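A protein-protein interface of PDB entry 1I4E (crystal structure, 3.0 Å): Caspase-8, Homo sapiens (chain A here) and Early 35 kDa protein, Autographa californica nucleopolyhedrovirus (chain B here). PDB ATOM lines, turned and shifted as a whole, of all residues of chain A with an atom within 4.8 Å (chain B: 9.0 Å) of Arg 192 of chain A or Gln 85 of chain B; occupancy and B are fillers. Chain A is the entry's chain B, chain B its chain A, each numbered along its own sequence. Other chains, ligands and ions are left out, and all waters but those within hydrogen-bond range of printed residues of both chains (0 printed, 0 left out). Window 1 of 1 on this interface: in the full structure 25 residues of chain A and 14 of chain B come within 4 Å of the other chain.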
ATOM      1  N   ARG A  37     -15.935   7.200 -27.096  1.00  0.00           N
ATOM      2  CA  ARG A  37     -15.150   5.988 -26.852  1.00  0.00           C
ATOM      3  C   ARG A  37     -14.514   6.049 -25.472  1.00  0.00           C
ATOM      4  O   ARG A  37     -14.686   7.022 -24.747  1.00  0.00           O
ATOM      5  CB  ARG A  37     -14.034   5.855 -27.889  1.00  0.00           C
ATOM      6  CG  ARG A  37     -14.490   5.717 -29.330  1.00  0.00           C
ATOM      7  CD  ARG A  37     -13.302   5.818 -30.286  1.00  0.00           C
ATOM      8  NE  ARG A  37     -12.269   4.816 -30.016  1.00  0.00           N
ATOM      9  CZ  ARG A  37     -11.119   4.728 -30.681  1.00  0.00           C
ATOM     10  NH1 ARG A  37     -10.850   5.583 -31.659  1.00  0.00           N
ATOM     11  NH2 ARG A  37     -10.237   3.784 -30.372  1.00  0.00           N
ATOM     12  N   ASP A  38     -13.778   5.008 -25.109  1.00  0.00           N
ATOM     13  CA  ASP A  38     -13.112   4.993 -23.818  1.00  0.00           C
ATOM     14  C   ASP A  38     -11.706   5.543 -23.986  1.00  0.00           C
ATOM     15  O   ASP A  38     -11.109   5.423 -25.054  1.00  0.00           O
ATOM     16  CB  ASP A  38     -13.078   3.574 -23.251  1.00  0.00           C
ATOM     17  CG  ASP A  38     -14.445   3.107 -22.795  1.00  0.00           C
ATOM     18  OD1 ASP A  38     -15.427   3.430 -23.490  1.00  0.00           O
ATOM     19  OD2 ASP A  38     -14.543   2.419 -21.757  1.00  0.00           O
ATOM     20  N   ARG A  39     -11.189   6.160 -22.925  1.00  0.00           N
ATOM     21  CA  ARG A  39      -9.854   6.755 -22.944  1.00  0.00           C
ATOM     22  C   ARG A  39      -8.772   5.700 -22.782  1.00  0.00           C
ATOM     23  O   ARG A  39      -8.170   5.594 -21.720  1.00  0.00           O
ATOM     24  CB  ARG A  39      -9.682   7.773 -21.807  1.00  0.00           C
ATOM     25  CG  ARG A  39     -10.802   8.774 -21.633  1.00  0.00           C
ATOM     26  CD  ARG A  39     -10.251  10.164 -21.398  1.00  0.00           C
ATOM     27  NE  ARG A  39      -9.171  10.195 -20.422  1.00  0.00           N
ATOM     28  CZ  ARG A  39      -8.005  10.794 -20.636  1.00  0.00           C
ATOM     29  NH1 ARG A  39      -7.768  11.409 -21.795  1.00  0.00           N
ATOM     30  NH2 ARG A  39      -7.082  10.780 -19.689  1.00  0.00           N
ATOM     31  N   ASN A  40      -8.521   4.926 -23.829  1.00  0.00           N
ATOM     32  CA  ASN A  40      -7.499   3.893 -23.769  1.00  0.00           C
ATOM     33  C   ASN A  40      -6.111   4.498 -23.706  1.00  0.00           C
ATOM     34  O   ASN A  40      -5.741   5.301 -24.553  1.00  0.00           O
ATOM     35  CB  ASN A  40      -7.603   2.981 -24.990  1.00  0.00           C
ATOM     36  CG  ASN A  40      -8.639   1.897 -24.811  1.00  0.00           C
ATOM     37  OD1 ASN A  40      -8.476   1.004 -23.980  1.00  0.00           O
ATOM     38  ND2 ASN A  40      -9.718   1.971 -25.584  1.00  0.00           N
ATOM     39  N   GLY A  41      -5.344   4.104 -22.699  1.00  0.00           N
ATOM     40  CA  GLY A  41      -4.001   4.626 -22.555  1.00  0.00           C
ATOM     41  C   GLY A  41      -3.804   5.415 -21.274  1.00  0.00           C
ATOM     42  O   GLY A  41      -2.686   5.506 -20.752  1.00  0.00           O
ATOM     43  N   THR A  42      -4.893   5.979 -20.766  1.00  0.00           N
ATOM     44  CA  THR A  42      -4.857   6.778 -19.549  1.00  0.00           C
ATOM     45  C   THR A  42      -3.994   6.112 -18.494  1.00  0.00           C
ATOM     46  O   THR A  42      -3.355   6.782 -17.682  1.00  0.00           O
ATOM     47  CB  THR A  42      -6.265   6.974 -18.965  1.00  0.00           C
ATOM     48  OG1 THR A  42      -7.239   6.747 -19.985  1.00  0.00           O
ATOM     49  CG2 THR A  42      -6.438   8.400 -18.470  1.00  0.00           C
ATOM     50  N   SER A 190      -7.626  18.136 -26.696  1.00  0.00           N
ATOM     51  CA  SER A 190      -6.393  17.604 -26.143  1.00  0.00           C
ATOM     52  C   SER A 190      -6.168  16.270 -26.844  1.00  0.00           C
ATOM     53  O   SER A 190      -7.114  15.645 -27.317  1.00  0.00           O
ATOM     54  CB  SER A 190      -6.508  17.378 -24.638  1.00  0.00           C
ATOM     55  OG  SER A 190      -5.408  16.615 -24.174  1.00  0.00           O
ATOM     56  N   TYR A 191      -4.917  15.836 -26.902  1.00  0.00           N
ATOM     57  CA  TYR A 191      -4.568  14.600 -27.582  1.00  0.00           C
ATOM     58  C   TYR A 191      -4.044  13.531 -26.647  1.00  0.00           C
ATOM     59  O   TYR A 191      -3.159  13.783 -25.833  1.00  0.00           O
ATOM     60  CB  TYR A 191      -3.524  14.896 -28.659  1.00  0.00           C
ATOM     61  CG  TYR A 191      -4.104  15.485 -29.930  1.00  0.00           C
ATOM     62  CD1 TYR A 191      -4.858  14.700 -30.783  1.00  0.00           C
ATOM     63  CD2 TYR A 191      -3.919  16.824 -30.264  1.00  0.00           C
ATOM     64  CE1 TYR A 191      -5.413  15.220 -31.932  1.00  0.00           C
ATOM     65  CE2 TYR A 191      -4.481  17.360 -31.420  1.00  0.00           C
ATOM     66  CZ  TYR A 191      -5.227  16.542 -32.248  1.00  0.00           C
ATOM     67  OH  TYR A 191      -5.804  17.007 -33.407  1.00  0.00           O
ATOM     68  N   ARG A 192      -4.608  12.334 -26.780  1.00  0.00           N
ATOM     69  CA  ARG A 192      -4.231  11.181 -25.976  1.00  0.00           C
ATOM     70  C   ARG A 192      -3.916  10.059 -26.937  1.00  0.00           C
ATOM     71  O   ARG A 192      -4.697   9.783 -27.844  1.00  0.00           O
ATOM     72  CB  ARG A 192      -5.389  10.755 -25.070  1.00  0.00           C
ATOM     73  CG  ARG A 192      -5.044   9.603 -24.143  1.00  0.00           C
ATOM     74  CD  ARG A 192      -6.256   9.066 -23.405  1.00  0.00           C
ATOM     75  NE  ARG A 192      -7.085   8.235 -24.269  1.00  0.00           N
ATOM     76  CZ  ARG A 192      -8.036   8.696 -25.073  1.00  0.00           C
ATOM     77  NH1 ARG A 192      -8.299   9.995 -25.131  1.00  0.00           N
ATOM     78  NH2 ARG A 192      -8.714   7.852 -25.836  1.00  0.00           N
ATOM     79  N   ASN A 193      -2.770   9.419 -26.741  1.00  0.00           N
ATOM     80  CA  ASN A 193      -2.359   8.328 -27.614  1.00  0.00           C
ATOM     81  C   ASN A 193      -2.437   6.987 -26.883  1.00  0.00           C
ATOM     82  O   ASN A 193      -1.858   6.815 -25.810  1.00  0.00           O
ATOM     83  CB  ASN A 193      -0.941   8.556 -28.120  1.00  0.00           C
ATOM     84  CG  ASN A 193      -0.499   7.470 -29.054  1.00  0.00           C
ATOM     85  OD1 ASN A 193      -0.719   7.549 -30.263  1.00  0.00           O
ATOM     86  ND2 ASN A 193       0.107   6.420 -28.498  1.00  0.00           N
ATOM     87  N   PRO A 194      -3.142   6.012 -27.474  1.00  0.00           N
ATOM     88  CA  PRO A 194      -3.311   4.682 -26.883  1.00  0.00           C
ATOM     89  C   PRO A 194      -2.053   3.915 -26.504  1.00  0.00           C
ATOM     90  O   PRO A 194      -2.014   3.252 -25.472  1.00  0.00           O
ATOM     91  CB  PRO A 194      -4.141   3.949 -27.930  1.00  0.00           C
ATOM     92  CG  PRO A 194      -3.733   4.602 -29.204  1.00  0.00           C
ATOM     93  CD  PRO A 194      -3.723   6.051 -28.827  1.00  0.00           C
ATOM     94  N   GLY A 197       0.797   7.483 -24.576  1.00  0.00           N
ATOM     95  CA  GLY A 197       0.134   8.247 -23.529  1.00  0.00           C
ATOM     96  C   GLY A 197      -0.334   9.576 -24.084  1.00  0.00           C
ATOM     97  O   GLY A 197      -0.301   9.780 -25.295  1.00  0.00           O
ATOM     98  N   THR A 198      -0.784  10.483 -23.224  1.00  0.00           N
ATOM     99  CA  THR A 198      -1.220  11.795 -23.699  1.00  0.00           C
ATOM    100  C   THR A 198       0.003  12.726 -23.796  1.00  0.00           C
ATOM    101  O   THR A 198       0.951  12.612 -23.024  1.00  0.00           O
ATOM    102  CB  THR A 198      -2.278  12.431 -22.760  1.00  0.00           C
ATOM    103  OG1 THR A 198      -1.635  12.980 -21.604  1.00  0.00           O
ATOM    104  CG2 THR A 198      -3.291  11.390 -22.313  1.00  0.00           C
ATOM    105  N   CYS B   2     -16.625  15.830 -27.843  1.00  0.00           N
ATOM    106  CA  CYS B   2     -15.866  15.021 -28.782  1.00  0.00           C
ATOM    107  C   CYS B   2     -16.438  15.065 -30.200  1.00  0.00           C
ATOM    108  O   CYS B   2     -17.315  14.285 -30.559  1.00  0.00           O
ATOM    109  CB  CYS B   2     -15.778  13.578 -28.270  1.00  0.00           C
ATOM    110  SG  CYS B   2     -17.002  13.158 -26.997  1.00  0.00           S
ATOM    111  N   VAL B   3     -15.913  16.001 -30.989  1.00  0.00           N
ATOM    112  CA  VAL B   3     -16.277  16.246 -32.389  1.00  0.00           C
ATOM    113  C   VAL B   3     -17.563  15.642 -32.965  1.00  0.00           C
ATOM    114  O   VAL B   3     -17.833  14.454 -32.809  1.00  0.00           O
ATOM    115  CB  VAL B   3     -15.095  15.852 -33.322  1.00  0.00           C
ATOM    116  CG1 VAL B   3     -14.732  14.382 -33.137  1.00  0.00           C
ATOM    117  CG2 VAL B   3     -15.449  16.162 -34.765  1.00  0.00           C
ATOM    118  N   ASP B  76     -11.946  -4.645 -36.928  1.00  0.00           N
ATOM    119  CA  ASP B  76     -11.165  -3.828 -36.023  1.00  0.00           C
ATOM    120  C   ASP B  76     -10.512  -4.647 -34.913  1.00  0.00           C
ATOM    121  O   ASP B  76      -9.570  -4.181 -34.272  1.00  0.00           O
ATOM    122  CB  ASP B  76     -12.058  -2.744 -35.416  1.00  0.00           C
ATOM    123  CG  ASP B  76     -11.277  -1.532 -34.958  1.00  0.00           C
ATOM    124  OD1 ASP B  76     -10.276  -1.710 -34.229  1.00  0.00           O
ATOM    125  OD2 ASP B  76     -11.673  -0.401 -35.328  1.00  0.00           O
ATOM    126  N   ARG B  80      -4.275  -3.025 -35.004  1.00  0.00           N
ATOM    127  CA  ARG B  80      -3.511  -2.552 -33.848  1.00  0.00           C
ATOM    128  C   ARG B  80      -3.130  -1.103 -34.107  1.00  0.00           C
ATOM    129  O   ARG B  80      -2.021  -0.676 -33.812  1.00  0.00           O
ATOM    130  CB  ARG B  80      -2.245  -3.377 -33.595  1.00  0.00           C
ATOM    131  CG  ARG B  80      -2.481  -4.722 -32.915  1.00  0.00           C
ATOM    132  CD  ARG B  80      -1.232  -5.192 -32.169  1.00  0.00           C
ATOM    133  NE  ARG B  80      -0.056  -5.306 -33.031  1.00  0.00           N
ATOM    134  CZ  ARG B  80       0.100  -6.212 -33.994  1.00  0.00           C
ATOM    135  NH1 ARG B  80      -0.847  -7.108 -34.238  1.00  0.00           N
ATOM    136  NH2 ARG B  80       1.212  -6.220 -34.714  1.00  0.00           N
ATOM    137  N   ASP B  81      -4.076  -0.364 -34.673  1.00  0.00           N
ATOM    138  CA  ASP B  81      -3.932   1.053 -34.993  1.00  0.00           C
ATOM    139  C   ASP B  81      -3.600   1.846 -33.736  1.00  0.00           C
ATOM    140  O   ASP B  81      -4.385   1.849 -32.789  1.00  0.00           O
ATOM    141  CB  ASP B  81      -5.253   1.550 -35.573  1.00  0.00           C
ATOM    142  CG  ASP B  81      -5.258   3.025 -35.834  1.00  0.00           C
ATOM    143  OD1 ASP B  81      -4.780   3.776 -34.959  1.00  0.00           O
ATOM    144  OD2 ASP B  81      -5.756   3.429 -36.906  1.00  0.00           O
ATOM    145  N   TYR B  82      -2.445   2.511 -33.728  1.00  0.00           N
ATOM    146  CA  TYR B  82      -2.022   3.306 -32.573  1.00  0.00           C
ATOM    147  C   TYR B  82      -2.074   4.818 -32.837  1.00  0.00           C
ATOM    148  O   TYR B  82      -1.369   5.607 -32.204  1.00  0.00           O
ATOM    149  CB  TYR B  82      -0.609   2.893 -32.114  1.00  0.00           C
ATOM    150  CG  TYR B  82      -0.488   1.450 -31.642  1.00  0.00           C
ATOM    151  CD1 TYR B  82      -1.618   0.709 -31.292  1.00  0.00           C
ATOM    152  CD2 TYR B  82       0.750   0.821 -31.571  1.00  0.00           C
ATOM    153  CE1 TYR B  82      -1.515  -0.624 -30.890  1.00  0.00           C
ATOM    154  CE2 TYR B  82       0.861  -0.507 -31.167  1.00  0.00           C
ATOM    155  CZ  TYR B  82      -0.269  -1.220 -30.832  1.00  0.00           C
ATOM    156  OH  TYR B  82      -0.156  -2.535 -30.461  1.00  0.00           O
ATOM    157  N   SER B  83      -2.927   5.214 -33.775  1.00  0.00           N
ATOM    158  CA  SER B  83      -3.103   6.619 -34.128  1.00  0.00           C
ATOM    159  C   SER B  83      -3.594   7.433 -32.928  1.00  0.00           C
ATOM    160  O   SER B  83      -4.319   6.921 -32.076  1.00  0.00           O
ATOM    161  CB  SER B  83      -4.127   6.739 -35.265  1.00  0.00           C
ATOM    162  OG  SER B  83      -3.689   6.068 -36.431  1.00  0.00           O
ATOM    163  N   ASP B  84      -3.209   8.703 -32.877  1.00  0.00           N
ATOM    164  CA  ASP B  84      -3.620   9.584 -31.794  1.00  0.00           C
ATOM    165  C   ASP B  84      -5.140   9.666 -31.705  1.00  0.00           C
ATOM    166  O   ASP B  84      -5.835   9.710 -32.726  1.00  0.00           O
ATOM    167  CB  ASP B  84      -3.045  10.986 -32.014  1.00  0.00           C
ATOM    168  CG  ASP B  84      -1.541  11.031 -31.841  1.00  0.00           C
ATOM    169  OD1 ASP B  84      -0.869  11.747 -32.617  1.00  0.00           O
ATOM    170  OD2 ASP B  84      -1.039  10.354 -30.918  1.00  0.00           O
ATOM    171  N   GLN B  85      -5.647   9.669 -30.475  1.00  0.00           N
ATOM    172  CA  GLN B  85      -7.082   9.775 -30.225  1.00  0.00           C
ATOM    173  C   GLN B  85      -7.318  11.086 -29.498  1.00  0.00           C
ATOM    174  O   GLN B  85      -6.393  11.868 -29.318  1.00  0.00           O
ATOM    175  CB  GLN B  85      -7.577   8.608 -29.375  1.00  0.00           C
ATOM    176  CG  GLN B  85      -7.806   7.338 -30.159  1.00  0.00           C
ATOM    177  CD  GLN B  85      -7.669   6.104 -29.303  1.00  0.00           C
ATOM    178  OE1 GLN B  85      -8.348   5.955 -28.280  1.00  0.00           O
ATOM    179  NE2 GLN B  85      -6.780   5.205 -29.714  1.00  0.00           N
ATOM    180  N   MET B  86      -8.550  11.332 -29.079  1.00  0.00           N
ATOM    181  CA  MET B  86      -8.848  12.577 -28.389  1.00  0.00           C
ATOM    182  C   MET B  86      -9.881  12.426 -27.286  1.00  0.00           C
ATOM    183  O   MET B  86     -10.323  11.318 -26.979  1.00  0.00           O
ATOM    184  CB  MET B  86      -9.351  13.618 -29.381  1.00  0.00           C
ATOM    185  CG  MET B  86      -8.353  14.053 -30.416  1.00  0.00           C
ATOM    186  SD  MET B  86      -9.068  15.394 -31.378  1.00  0.00           S
ATOM    187  CE  MET B  86     -10.096  14.469 -32.509  1.00  0.00           C
ATOM    188  N   ASP B  87     -10.246  13.565 -26.698  1.00  0.00           N
ATOM    189  CA  ASP B  87     -11.242  13.643 -25.637  1.00  0.00           C
ATOM    190  C   ASP B  87     -12.207  14.739 -26.098  1.00  0.00           C
ATOM    191  O   ASP B  87     -13.341  14.466 -26.492  1.00  0.00           O
ATOM    192  CB  ASP B  87     -10.579  14.041 -24.305  1.00  0.00           C
ATOM    193  CG  ASP B  87      -9.436  13.088 -23.892  1.00  0.00           C
ATOM    194  OD1 ASP B  87      -9.685  11.918 -23.562  1.00  0.00           O
ATOM    195  OD2 ASP B  87      -8.265  13.498 -23.891  1.00  0.00           O
ATOM    196  N   TRP B 262       2.539  -1.967 -35.437  1.00  0.00           N
ATOM    197  CA  TRP B 262       1.263  -1.670 -36.038  1.00  0.00           C
ATOM    198  C   TRP B 262       0.761  -2.796 -36.917  1.00  0.00           C
ATOM    199  O   TRP B 262       1.509  -3.691 -37.298  1.00  0.00           O
ATOM    200  CB  TRP B 262       1.380  -0.394 -36.858  1.00  0.00           C
ATOM    201  CG  TRP B 262       1.582   0.807 -36.017  1.00  0.00           C
ATOM    202  CD1 TRP B 262       2.508   0.971 -35.028  1.00  0.00           C
ATOM    203  CD2 TRP B 262       0.840   2.024 -36.081  1.00  0.00           C
ATOM    204  NE1 TRP B 262       2.385   2.220 -34.471  1.00  0.00           N
ATOM    205  CE2 TRP B 262       1.367   2.887 -35.097  1.00  0.00           C
ATOM    206  CE3 TRP B 262      -0.223   2.471 -36.874  1.00  0.00           C
ATOM    207  CZ2 TRP B 262       0.869   4.174 -34.889  1.00  0.00           C
ATOM    208  CZ3 TRP B 262      -0.716   3.748 -36.668  1.00  0.00           C
ATOM    209  CH2 TRP B 262      -0.172   4.584 -35.682  1.00  0.00           C
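Gln 85 of chain B touches just these residues of chain A: Arg 37 (3.6 Å), Tyr 191 (3.5 Å), Arg 192 (2.8 Å) and Pro 194 (3.1 Å). Arg 39 of chain A touches one residue of chain B. Printed residues of chain B within 4 Å of Pro 194 of chain A: Tyr 82, Ser 83 and Gln 85. Of the printed residues of chain A, Tyr 82 of chain B touches Asn 193 and Pro 194. Of the printed residues of chain B, Tyr 191 of chain A touches Gln 85 (3.5 Å) and Met 86 (3.5 Å). Printed residues of chain B within 4 Å of Arg 37 of chain A: Gln 85 (3.6 Å). Trp 262 of chain B touches none of the printed residues of chain A. Gly 41 of chain A touches none of the printed residues of chain B. The nearest residue of chain A that does not touch Gln 85 of chain B is Asp 38 of chain A (4.3 Å).
Hydrophobic or aromatic side chains of chain A that line the printed part of chain B: Tyr 191 and Pro 194.
OD1 of Asn 193 of chain A sits close to O of Tyr 82 of chain B, 2.8 Å away. The side-chain carboxylate (OD2) of Asp 84 of chain B sits close to the side-chain amide oxygen (OD1) of Asn 193 of chain A (2.9 Å). The guanidinium group (NH1) of Arg 192 of chain A lies within salt-bridge range of the side-chain carboxylate (OD1) of Asp 87 of chain B, at 2.8 Å. NH1 of Arg 39 of chain A is in salt-bridge range of OD1 of Asp 87 of chain B (2.7 Å). The backbone NH (N) of Gln 85 of chain B sits at hydrogen-bond distance from the backbone carbonyl oxygen (O) of Arg 192 of chain A (2.8 Å). The guanidinium group (NH1) of Arg 192 of chain A lies within hydrogen-bond range of the backbone carbonyl oxygen (O) of Met 86 of chain B (3.0 Å).
OD1 of Asp 81 of chain B lies within hydrogen-bond range of N of Ser 83 of chain B (2.6 Å). The backbone carbonyl oxygen of Asp 38 of chain A sits at hydrogen-bond distance from the guanidinium group of Arg 192 of chain A. The backbone carbonyl oxygen of Asn 40 of chain A is in hydrogen-bond range of the guanidinium group of Arg 192 of chain A (3.2 Å).
Among the printed residues, merely in contact across the chains: Pro 194 of chain A with Gln 85 of chain B (3.1 Å), Pro 194 of chain A with Ser 83 of chain B (3.4 Å), Tyr 191 of chain A with Met 86 of chain B (3.5 Å), Tyr 191 of chain A with Gln 85 of chain B (3.5 Å), Arg 37 of chain A with Gln 85 of chain B (3.6 Å), Ser 190 of chain A with Met 86 of chain B (3.7 Å), Ser 190 of chain A with Asp 87 of chain B (3.8 Å), Arg 192 of chain A with Asp 84 of chain B (3.9 Å), Asn 193 of chain A with Ser 83 of chain B (3.9 Å) and Pro 194 of chain A with Tyr 82 of chain B (3.9 Å).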
